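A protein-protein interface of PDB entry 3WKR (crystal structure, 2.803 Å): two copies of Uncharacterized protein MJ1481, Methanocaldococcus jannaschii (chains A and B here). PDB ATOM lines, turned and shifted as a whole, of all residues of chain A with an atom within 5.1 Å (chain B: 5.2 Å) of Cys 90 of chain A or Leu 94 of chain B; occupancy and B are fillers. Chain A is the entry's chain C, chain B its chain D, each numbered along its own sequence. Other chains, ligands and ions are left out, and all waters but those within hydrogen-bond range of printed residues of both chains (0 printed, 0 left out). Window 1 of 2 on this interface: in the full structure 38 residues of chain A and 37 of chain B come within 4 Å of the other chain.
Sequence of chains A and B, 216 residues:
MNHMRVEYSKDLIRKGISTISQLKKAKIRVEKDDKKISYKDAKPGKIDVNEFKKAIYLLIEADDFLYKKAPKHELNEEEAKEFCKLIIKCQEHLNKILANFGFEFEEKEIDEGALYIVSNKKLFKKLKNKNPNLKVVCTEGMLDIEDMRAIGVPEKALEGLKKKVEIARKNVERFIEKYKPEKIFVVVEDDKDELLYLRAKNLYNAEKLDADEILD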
ATOM      1  N   ALA A  55      10.213 -25.629   0.240  1.00  0.00           N
ATOM      2  CA  ALA A  55      10.759 -25.454   1.581  1.00  0.00           C
ATOM      3  C   ALA A  55       9.772 -25.937   2.637  1.00  0.00           C
ATOM      4  O   ALA A  55      10.166 -26.483   3.669  1.00  0.00           O
ATOM      5  CB  ALA A  55      11.123 -23.997   1.820  1.00  0.00           C
ATOM      6  N   LEU A  58       9.534 -29.926   2.809  1.00  0.00           N
ATOM      7  CA  LEU A  58      10.662 -30.536   3.503  1.00  0.00           C
ATOM      8  C   LEU A  58      10.459 -30.541   5.014  1.00  0.00           C
ATOM      9  O   LEU A  58      10.851 -31.488   5.696  1.00  0.00           O
ATOM     10  CB  LEU A  58      11.964 -29.823   3.136  1.00  0.00           C
ATOM     11  CG  LEU A  58      12.423 -30.046   1.694  1.00  0.00           C
ATOM     12  CD1 LEU A  58      13.514 -29.062   1.318  1.00  0.00           C
ATOM     13  CD2 LEU A  58      12.900 -31.478   1.503  1.00  0.00           C
ATOM     14  N   LEU A  59       9.844 -29.484   5.534  1.00  0.00           N
ATOM     15  CA  LEU A  59       9.524 -29.416   6.956  1.00  0.00           C
ATOM     16  C   LEU A  59       8.362 -30.344   7.286  1.00  0.00           C
ATOM     17  O   LEU A  59       8.219 -30.798   8.421  1.00  0.00           O
ATOM     18  CB  LEU A  59       9.189 -27.984   7.377  1.00  0.00           C
ATOM     19  CG  LEU A  59      10.337 -26.973   7.344  1.00  0.00           C
ATOM     20  CD1 LEU A  59       9.889 -25.638   7.917  1.00  0.00           C
ATOM     21  CD2 LEU A  59      11.551 -27.505   8.093  1.00  0.00           C
ATOM     22  N   LYS A  85      19.482 -33.749   6.171  1.00  0.00           N
ATOM     23  CA  LYS A  85      19.406 -33.602   4.722  1.00  0.00           C
ATOM     24  C   LYS A  85      18.198 -32.759   4.336  1.00  0.00           C
ATOM     25  O   LYS A  85      18.259 -31.951   3.411  1.00  0.00           O
ATOM     26  CB  LYS A  85      19.323 -34.975   4.050  1.00  0.00           C
ATOM     27  CG  LYS A  85      19.296 -34.940   2.532  1.00  0.00           C
ATOM     28  CD  LYS A  85      19.239 -36.347   1.958  1.00  0.00           C
ATOM     29  CE  LYS A  85      19.258 -36.330   0.439  1.00  0.00           C
ATOM     30  NZ  LYS A  85      19.225 -37.706  -0.132  1.00  0.00           N
ATOM     31  N   LEU A  86      17.101 -32.950   5.061  1.00  0.00           N
ATOM     32  CA  LEU A  86      15.870 -32.214   4.808  1.00  0.00           C
ATOM     33  C   LEU A  86      15.989 -30.757   5.246  1.00  0.00           C
ATOM     34  O   LEU A  86      15.538 -29.850   4.545  1.00  0.00           O
ATOM     35  CB  LEU A  86      14.699 -32.886   5.528  1.00  0.00           C
ATOM     36  CG  LEU A  86      14.438 -34.345   5.144  1.00  0.00           C
ATOM     37  CD1 LEU A  86      13.501 -35.006   6.142  1.00  0.00           C
ATOM     38  CD2 LEU A  86      13.873 -34.435   3.733  1.00  0.00           C
ATOM     39  N   ILE A  87      16.599 -30.539   6.407  1.00  0.00           N
ATOM     40  CA  ILE A  87      16.738 -29.197   6.963  1.00  0.00           C
ATOM     41  C   ILE A  87      17.732 -28.360   6.161  1.00  0.00           C
ATOM     42  O   ILE A  87      17.532 -27.159   5.969  1.00  0.00           O
ATOM     43  CB  ILE A  87      17.168 -29.246   8.444  1.00  0.00           C
ATOM     44  CG1 ILE A  87      16.269 -30.203   9.229  1.00  0.00           C
ATOM     45  CG2 ILE A  87      17.135 -27.855   9.061  1.00  0.00           C
ATOM     46  CD1 ILE A  87      14.806 -29.813   9.224  1.00  0.00           C
ATOM     47  N   ILE A  88      18.799 -28.999   5.691  1.00  0.00           N
ATOM     48  CA  ILE A  88      19.788 -28.330   4.850  1.00  0.00           C
ATOM     49  C   ILE A  88      19.174 -27.931   3.511  1.00  0.00           C
ATOM     50  O   ILE A  88      19.387 -26.817   3.027  1.00  0.00           O
ATOM     51  CB  ILE A  88      21.036 -29.212   4.624  1.00  0.00           C
ATOM     52  CG1 ILE A  88      21.845 -29.325   5.918  1.00  0.00           C
ATOM     53  CG2 ILE A  88      21.906 -28.642   3.514  1.00  0.00           C
ATOM     54  CD1 ILE A  88      23.083 -30.185   5.795  1.00  0.00           C
ATOM     55  N   LYS A  89      18.403 -28.840   2.923  1.00  0.00           N
ATOM     56  CA  LYS A  89      17.698 -28.550   1.678  1.00  0.00           C
ATOM     57  C   LYS A  89      16.640 -27.471   1.884  1.00  0.00           C
ATOM     58  O   LYS A  89      16.353 -26.691   0.976  1.00  0.00           O
ATOM     59  CB  LYS A  89      17.050 -29.816   1.113  1.00  0.00           C
ATOM     60  CG  LYS A  89      18.024 -30.788   0.472  1.00  0.00           C
ATOM     61  CD  LYS A  89      17.311 -32.048   0.009  1.00  0.00           C
ATOM     62  CE  LYS A  89      18.272 -33.007  -0.671  1.00  0.00           C
ATOM     63  NZ  LYS A  89      18.876 -32.413  -1.895  1.00  0.00           N
ATOM     64  N   CYS A  90      16.066 -27.429   3.082  1.00  0.00           N
ATOM     65  CA  CYS A  90      15.044 -26.440   3.411  1.00  0.00           C
ATOM     66  C   CYS A  90      15.618 -25.027   3.424  1.00  0.00           C
ATOM     67  O   CYS A  90      15.067 -24.120   2.799  1.00  0.00           O
ATOM     68  CB  CYS A  90      14.399 -26.755   4.761  1.00  0.00           C
ATOM     69  SG  CYS A  90      13.106 -25.591   5.258  1.00  0.00           S
ATOM     70  N   GLN A  91      16.722 -24.847   4.141  1.00  0.00           N
ATOM     71  CA  GLN A  91      17.392 -23.554   4.211  1.00  0.00           C
ATOM     72  C   GLN A  91      17.944 -23.147   2.851  1.00  0.00           C
ATOM     73  O   GLN A  91      17.991 -21.961   2.520  1.00  0.00           O
ATOM     74  CB  GLN A  91      18.523 -23.586   5.241  1.00  0.00           C
ATOM     75  CG  GLN A  91      18.057 -23.584   6.685  1.00  0.00           C
ATOM     76  CD  GLN A  91      19.213 -23.540   7.665  1.00  0.00           C
ATOM     77  OE1 GLN A  91      20.255 -24.154   7.438  1.00  0.00           O
ATOM     78  NE2 GLN A  91      19.035 -22.808   8.757  1.00  0.00           N
ATOM     79  N   GLU A  92      18.365 -24.137   2.070  1.00  0.00           N
ATOM     80  CA  GLU A  92      18.890 -23.895   0.731  1.00  0.00           C
ATOM     81  C   GLU A  92      17.810 -23.302  -0.168  1.00  0.00           C
ATOM     82  O   GLU A  92      18.096 -22.479  -1.039  1.00  0.00           O
ATOM     83  CB  GLU A  92      19.435 -25.192   0.127  1.00  0.00           C
ATOM     84  CG  GLU A  92      20.077 -25.021  -1.241  1.00  0.00           C
ATOM     85  CD  GLU A  92      20.642 -26.320  -1.785  1.00  0.00           C
ATOM     86  OE1 GLU A  92      21.012 -26.354  -2.978  1.00  0.00           O
ATOM     87  OE2 GLU A  92      20.719 -27.304  -1.020  1.00  0.00           O
ATOM     88  N   HIS A  93      16.568 -23.723   0.050  1.00  0.00           N
ATOM     89  CA  HIS A  93      15.436 -23.173  -0.687  1.00  0.00           C
ATOM     90  C   HIS A  93      15.067 -21.788  -0.164  1.00  0.00           C
ATOM     91  O   HIS A  93      14.681 -20.908  -0.934  1.00  0.00           O
ATOM     92  CB  HIS A  93      14.228 -24.110  -0.612  1.00  0.00           C
ATOM     93  CG  HIS A  93      14.327 -25.298  -1.518  1.00  0.00           C
ATOM     94  ND1 HIS A  93      14.439 -25.182  -2.886  1.00  0.00           N
ATOM     95  CD2 HIS A  93      14.324 -26.626  -1.252  1.00  0.00           C
ATOM     96  CE1 HIS A  93      14.505 -26.387  -3.424  1.00  0.00           C
ATOM     97  NE2 HIS A  93      14.438 -27.280  -2.455  1.00  0.00           N
ATOM     98  N   LEU A  94      15.193 -21.601   1.146  1.00  0.00           N
ATOM     99  CA  LEU A  94      14.889 -20.316   1.768  1.00  0.00           C
ATOM    100  C   LEU A  94      15.910 -19.251   1.380  1.00  0.00           C
ATOM    101  O   LEU A  94      15.583 -18.067   1.297  1.00  0.00           O
ATOM    102  CB  LEU A  94      14.818 -20.451   3.291  1.00  0.00           C
ATOM    103  CG  LEU A  94      13.647 -21.251   3.864  1.00  0.00           C
ATOM    104  CD1 LEU A  94      13.699 -21.258   5.383  1.00  0.00           C
ATOM    105  CD2 LEU A  94      12.320 -20.690   3.373  1.00  0.00           C
ATOM    106  N   PHE B  52      11.827 -26.608  16.158  1.00  0.00           N
ATOM    107  CA  PHE B  52      11.239 -27.048  14.898  1.00  0.00           C
ATOM    108  C   PHE B  52       9.825 -26.502  14.759  1.00  0.00           C
ATOM    109  O   PHE B  52       9.380 -26.175  13.659  1.00  0.00           O
ATOM    110  CB  PHE B  52      11.225 -28.576  14.808  1.00  0.00           C
ATOM    111  CG  PHE B  52      10.665 -29.102  13.515  1.00  0.00           C
ATOM    112  CD1 PHE B  52      11.470 -29.223  12.396  1.00  0.00           C
ATOM    113  CD2 PHE B  52       9.333 -29.478  13.420  1.00  0.00           C
ATOM    114  CE1 PHE B  52      10.961 -29.706  11.205  1.00  0.00           C
ATOM    115  CE2 PHE B  52       8.818 -29.961  12.232  1.00  0.00           C
ATOM    116  CZ  PHE B  52       9.634 -30.075  11.124  1.00  0.00           C
ATOM    117  N   ALA B  55      10.250 -22.895  13.902  1.00  0.00           N
ATOM    118  CA  ALA B  55      10.742 -22.784  12.535  1.00  0.00           C
ATOM    119  C   ALA B  55       9.627 -23.020  11.523  1.00  0.00           C
ATOM    120  O   ALA B  55       9.595 -22.392  10.465  1.00  0.00           O
ATOM    121  CB  ALA B  55      11.884 -23.761  12.301  1.00  0.00           C
ATOM    122  N   LEU B  59       7.172 -20.142   8.906  1.00  0.00           N
ATOM    123  CA  LEU B  59       6.919 -20.403   7.494  1.00  0.00           C
ATOM    124  C   LEU B  59       5.421 -20.406   7.198  1.00  0.00           C
ATOM    125  O   LEU B  59       5.001 -20.175   6.065  1.00  0.00           O
ATOM    126  CB  LEU B  59       7.565 -21.722   7.059  1.00  0.00           C
ATOM    127  CG  LEU B  59       8.539 -21.616   5.882  1.00  0.00           C
ATOM    128  CD1 LEU B  59       9.637 -20.604   6.178  1.00  0.00           C
ATOM    129  CD2 LEU B  59       9.136 -22.974   5.543  1.00  0.00           C
ATOM    130  N   CYS B  90      13.504 -17.927  10.686  1.00  0.00           N
ATOM    131  CA  CYS B  90      13.250 -19.346  10.463  1.00  0.00           C
ATOM    132  C   CYS B  90      14.557 -20.120  10.352  1.00  0.00           C
ATOM    133  O   CYS B  90      14.713 -21.179  10.959  1.00  0.00           O
ATOM    134  CB  CYS B  90      12.413 -19.555   9.199  1.00  0.00           C
ATOM    135  SG  CYS B  90      12.138 -21.291   8.766  1.00  0.00           S
ATOM    136  N   GLN B  91      15.492 -19.584   9.575  1.00  0.00           N
ATOM    137  CA  GLN B  91      16.797 -20.210   9.405  1.00  0.00           C
ATOM    138  C   GLN B  91      17.586 -20.200  10.708  1.00  0.00           C
ATOM    139  O   GLN B  91      18.418 -21.074  10.945  1.00  0.00           O
ATOM    140  CB  GLN B  91      17.592 -19.515   8.297  1.00  0.00           C
ATOM    141  CG  GLN B  91      17.041 -19.751   6.901  1.00  0.00           C
ATOM    142  CD  GLN B  91      17.869 -19.075   5.829  1.00  0.00           C
ATOM    143  OE1 GLN B  91      18.600 -18.123   6.099  1.00  0.00           O
ATOM    144  NE2 GLN B  91      17.762 -19.569   4.601  1.00  0.00           N
ATOM    145  N   GLU B  92      17.319 -19.209  11.553  1.00  0.00           N
ATOM    146  CA  GLU B  92      17.966 -19.132  12.859  1.00  0.00           C
ATOM    147  C   GLU B  92      17.477 -20.247  13.780  1.00  0.00           C
ATOM    148  O   GLU B  92      18.189 -20.663  14.693  1.00  0.00           O
ATOM    149  CB  GLU B  92      17.732 -17.765  13.507  1.00  0.00           C
ATOM    150  CG  GLU B  92      18.470 -16.623  12.827  1.00  0.00           C
ATOM    151  CD  GLU B  92      18.449 -15.349  13.647  1.00  0.00           C
ATOM    152  OE1 GLU B  92      17.923 -15.377  14.779  1.00  0.00           O
ATOM    153  OE2 GLU B  92      18.961 -14.319  13.160  1.00  0.00           O
ATOM    154  N   HIS B  93      16.262 -20.726  13.533  1.00  0.00           N
ATOM    155  CA  HIS B  93      15.719 -21.849  14.289  1.00  0.00           C
ATOM    156  C   HIS B  93      16.176 -23.170  13.684  1.00  0.00           C
ATOM    157  O   HIS B  93      16.429 -24.136  14.403  1.00  0.00           O
ATOM    158  CB  HIS B  93      14.190 -21.793  14.332  1.00  0.00           C
ATOM    159  CG  HIS B  93      13.649 -20.685  15.179  1.00  0.00           C
ATOM    160  ND1 HIS B  93      13.813 -20.647  16.548  1.00  0.00           N
ATOM    161  CD2 HIS B  93      12.938 -19.581  14.856  1.00  0.00           C
ATOM    162  CE1 HIS B  93      13.230 -19.563  17.028  1.00  0.00           C
ATOM    163  NE2 HIS B  93      12.693 -18.898  16.022  1.00  0.00           N
ATOM    164  N   LEU B  94      16.284 -23.206  12.360  1.00  0.00           N
ATOM    165  CA  LEU B  94      16.735 -24.405  11.662  1.00  0.00           C
ATOM    166  C   LEU B  94      18.220 -24.663  11.897  1.00  0.00           C
ATOM    167  O   LEU B  94      18.666 -25.810  11.882  1.00  0.00           O
ATOM    168  CB  LEU B  94      16.443 -24.307  10.163  1.00  0.00           C
ATOM    169  CG  LEU B  94      14.968 -24.363   9.763  1.00  0.00           C
ATOM    170  CD1 LEU B  94      14.808 -24.234   8.254  1.00  0.00           C
ATOM    171  CD2 LEU B  94      14.326 -25.648  10.266  1.00  0.00           C
ATOM    172  N   ASN B  95      18.980 -23.594  12.110  1.00  0.00           N
ATOM    173  CA  ASN B  95      20.398 -23.723  12.426  1.00  0.00           C
ATOM    174  C   ASN B  95      20.612 -24.289  13.824  1.00  0.00           C
ATOM    175  O   ASN B  95      21.561 -25.036  14.063  1.00  0.00           O
ATOM    176  CB  ASN B  95      21.114 -22.377  12.285  1.00  0.00           C
ATOM    177  CG  ASN B  95      21.304 -21.967  10.839  1.00  0.00           C
ATOM    178  OD1 ASN B  95      21.324 -22.808   9.941  1.00  0.00           O
ATOM    179  ND2 ASN B  95      21.447 -20.667  10.605  1.00  0.00           N
ATOM    180  N   LYS B  96      19.722 -23.931  14.745  1.00  0.00           N
ATOM    181  CA  LYS B  96      19.789 -24.436  16.111  1.00  0.00           C
ATOM    182  C   LYS B  96      19.453 -25.921  16.162  1.00  0.00           C
ATOM    183  O   LYS B  96      19.920 -26.643  17.042  1.00  0.00           O
ATOM    184  CB  LYS B  96      18.850 -23.650  17.029  1.00  0.00           C
ATOM    185  CG  LYS B  96      19.281 -22.216  17.272  1.00  0.00           C
ATOM    186  CD  LYS B  96      18.341 -21.512  18.235  1.00  0.00           C
ATOM    187  CE  LYS B  96      18.726 -20.053  18.414  1.00  0.00           C
ATOM    188  NZ  LYS B  96      18.585 -19.285  17.147  1.00  0.00           N
ATOM    189  N   ILE B  97      18.636 -26.368  15.213  1.00  0.00           N
ATOM    190  CA  ILE B  97      18.296 -27.781  15.102  1.00  0.00           C
ATOM    191  C   ILE B  97      19.508 -28.582  14.634  1.00  0.00           C
ATOM    192  O   ILE B  97      19.808 -29.647  15.172  1.00  0.00           O
ATOM    193  CB  ILE B  97      17.132 -28.005  14.119  1.00  0.00           C
ATOM    194  CG1 ILE B  97      15.865 -27.316  14.623  1.00  0.00           C
ATOM    195  CG2 ILE B  97      16.877 -29.489  13.925  1.00  0.00           C
ATOM    196  CD1 ILE B  97      14.665 -27.521  13.724  1.00  0.00           C
ATOM    197  N   LEU B  98      20.204 -28.052  13.634  1.00  0.00           N
ATOM    198  CA  LEU B  98      21.375 -28.716  13.070  1.00  0.00           C
ATOM    199  C   LEU B  98      22.552 -28.718  14.042  1.00  0.00           C
ATOM    200  O   LEU B  98      23.493 -29.495  13.886  1.00  0.00           O
ATOM    201  CB  LEU B  98      21.787 -28.045  11.758  1.00  0.00           C
ATOM    202  CG  LEU B  98      20.750 -28.057  10.634  1.00  0.00           C
ATOM    203  CD1 LEU B  98      21.291 -27.359   9.396  1.00  0.00           C
ATOM    204  CD2 LEU B  98      20.334 -29.483  10.313  1.00  0.00           C
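O of Ala 55 of chain A sits at hydrogen-bond distance from SG of Cys 90 of chain A (3.5 Å). O of Ala 55 of chain B lies within hydrogen-bond range of SG of Cys 90 of chain B, 3.3 Å away. The backbone carbonyl oxygen of Gln 91 of chain B lies close to the side-chain amide nitrogen of Asn 95 of chain B.
Leu 59 of chain B touches its own counterpart, Leu 59 of chain A. Leu 59 of chain A touches Leu 94 of chain B, and with the chains exchanged Leu 94 of chain A touches Leu 59 of chain B. Gln 91 of chain A touches its own counterpart, Gln 91 of chain B. Gln 91 of chain A touches Leu 94 of chain B, and with the chains exchanged Leu 94 of chain A touches Gln 91 of chain B. Of the 13 pairs that touch across the chains among the printed residues, 8 have their exchanged pair printed and touching as well.
Of the 13 printed residues of chain A, 5 touch a printed residue of chain B. Hydrophobic or aromatic side chains of chain A within 4 Å of the printed part of chain B: Leu 59, Ile 87 and Leu 94. Along chain A the printed residues that touch a printed residue of chain B span positions 59 to 94. Printed residues of chain B that touch a printed residue of chain A: Phe 52, Leu 59, Cys 90, Gln 91, Leu 94, Asn 95 and Leu 98.
The side-chain amide nitrogen (NE2) of Gln 91 of chain A lies within hydrogen-bond range of the backbone carbonyl oxygen (O) of Gln 91 of chain B. The side-chain amide oxygen (OD1) of Asn 95 of chain B sits at hydrogen-bond distance from the side-chain amide nitrogen (NE2) of Gln 91 of chain A (2.6 Å).
Among the printed residues, pairs that only touch across the chains: Leu 59 of chain A with Phe 52 of chain B (3.1 Å), Leu 59 of chain A with Leu 59 of chain B (3.6 Å), Leu 59 of chain A with Leu 94 of chain B (3.98 Å), Ile 87 of chain A with Leu 94 of chain B (3.8 Å), Ile 87 of chain A with Leu 98 of chain B (3.7 Å), Cys 90 of chain A with Leu 94 of chain B (3.7 Å), Gln 91 of chain A with Leu 94 of chain B (3.3 Å), Gln 91 of chain A with Leu 98 of chain B (3.9 Å), Leu 94 of chain A with Leu 59 of chain B (3.9 Å), Leu 94 of chain A with Cys 90 of chain B (3.7 Å) and Leu 94 of chain A with Gln 91 of chain B (3.3 Å).
Of the printed residues of chain A, Leu 98 of chain B touches Ile 87 and Gln 91. Printed residues of chain A within 4 Å of Asn 95 of chain B: Gln 91. Glu 92 of chain B touches none of the printed residues of chain A. His 93 of chain A touches none of the printed residues of chain B. The nearest residue of chain B that does not touch Cys 90 of chain A is Leu 59 of chain B (4.8 Å). The nearest printed residue of chain A that does not touch Leu 94 of chain B is Leu 94 of chain A (4.3 Å).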
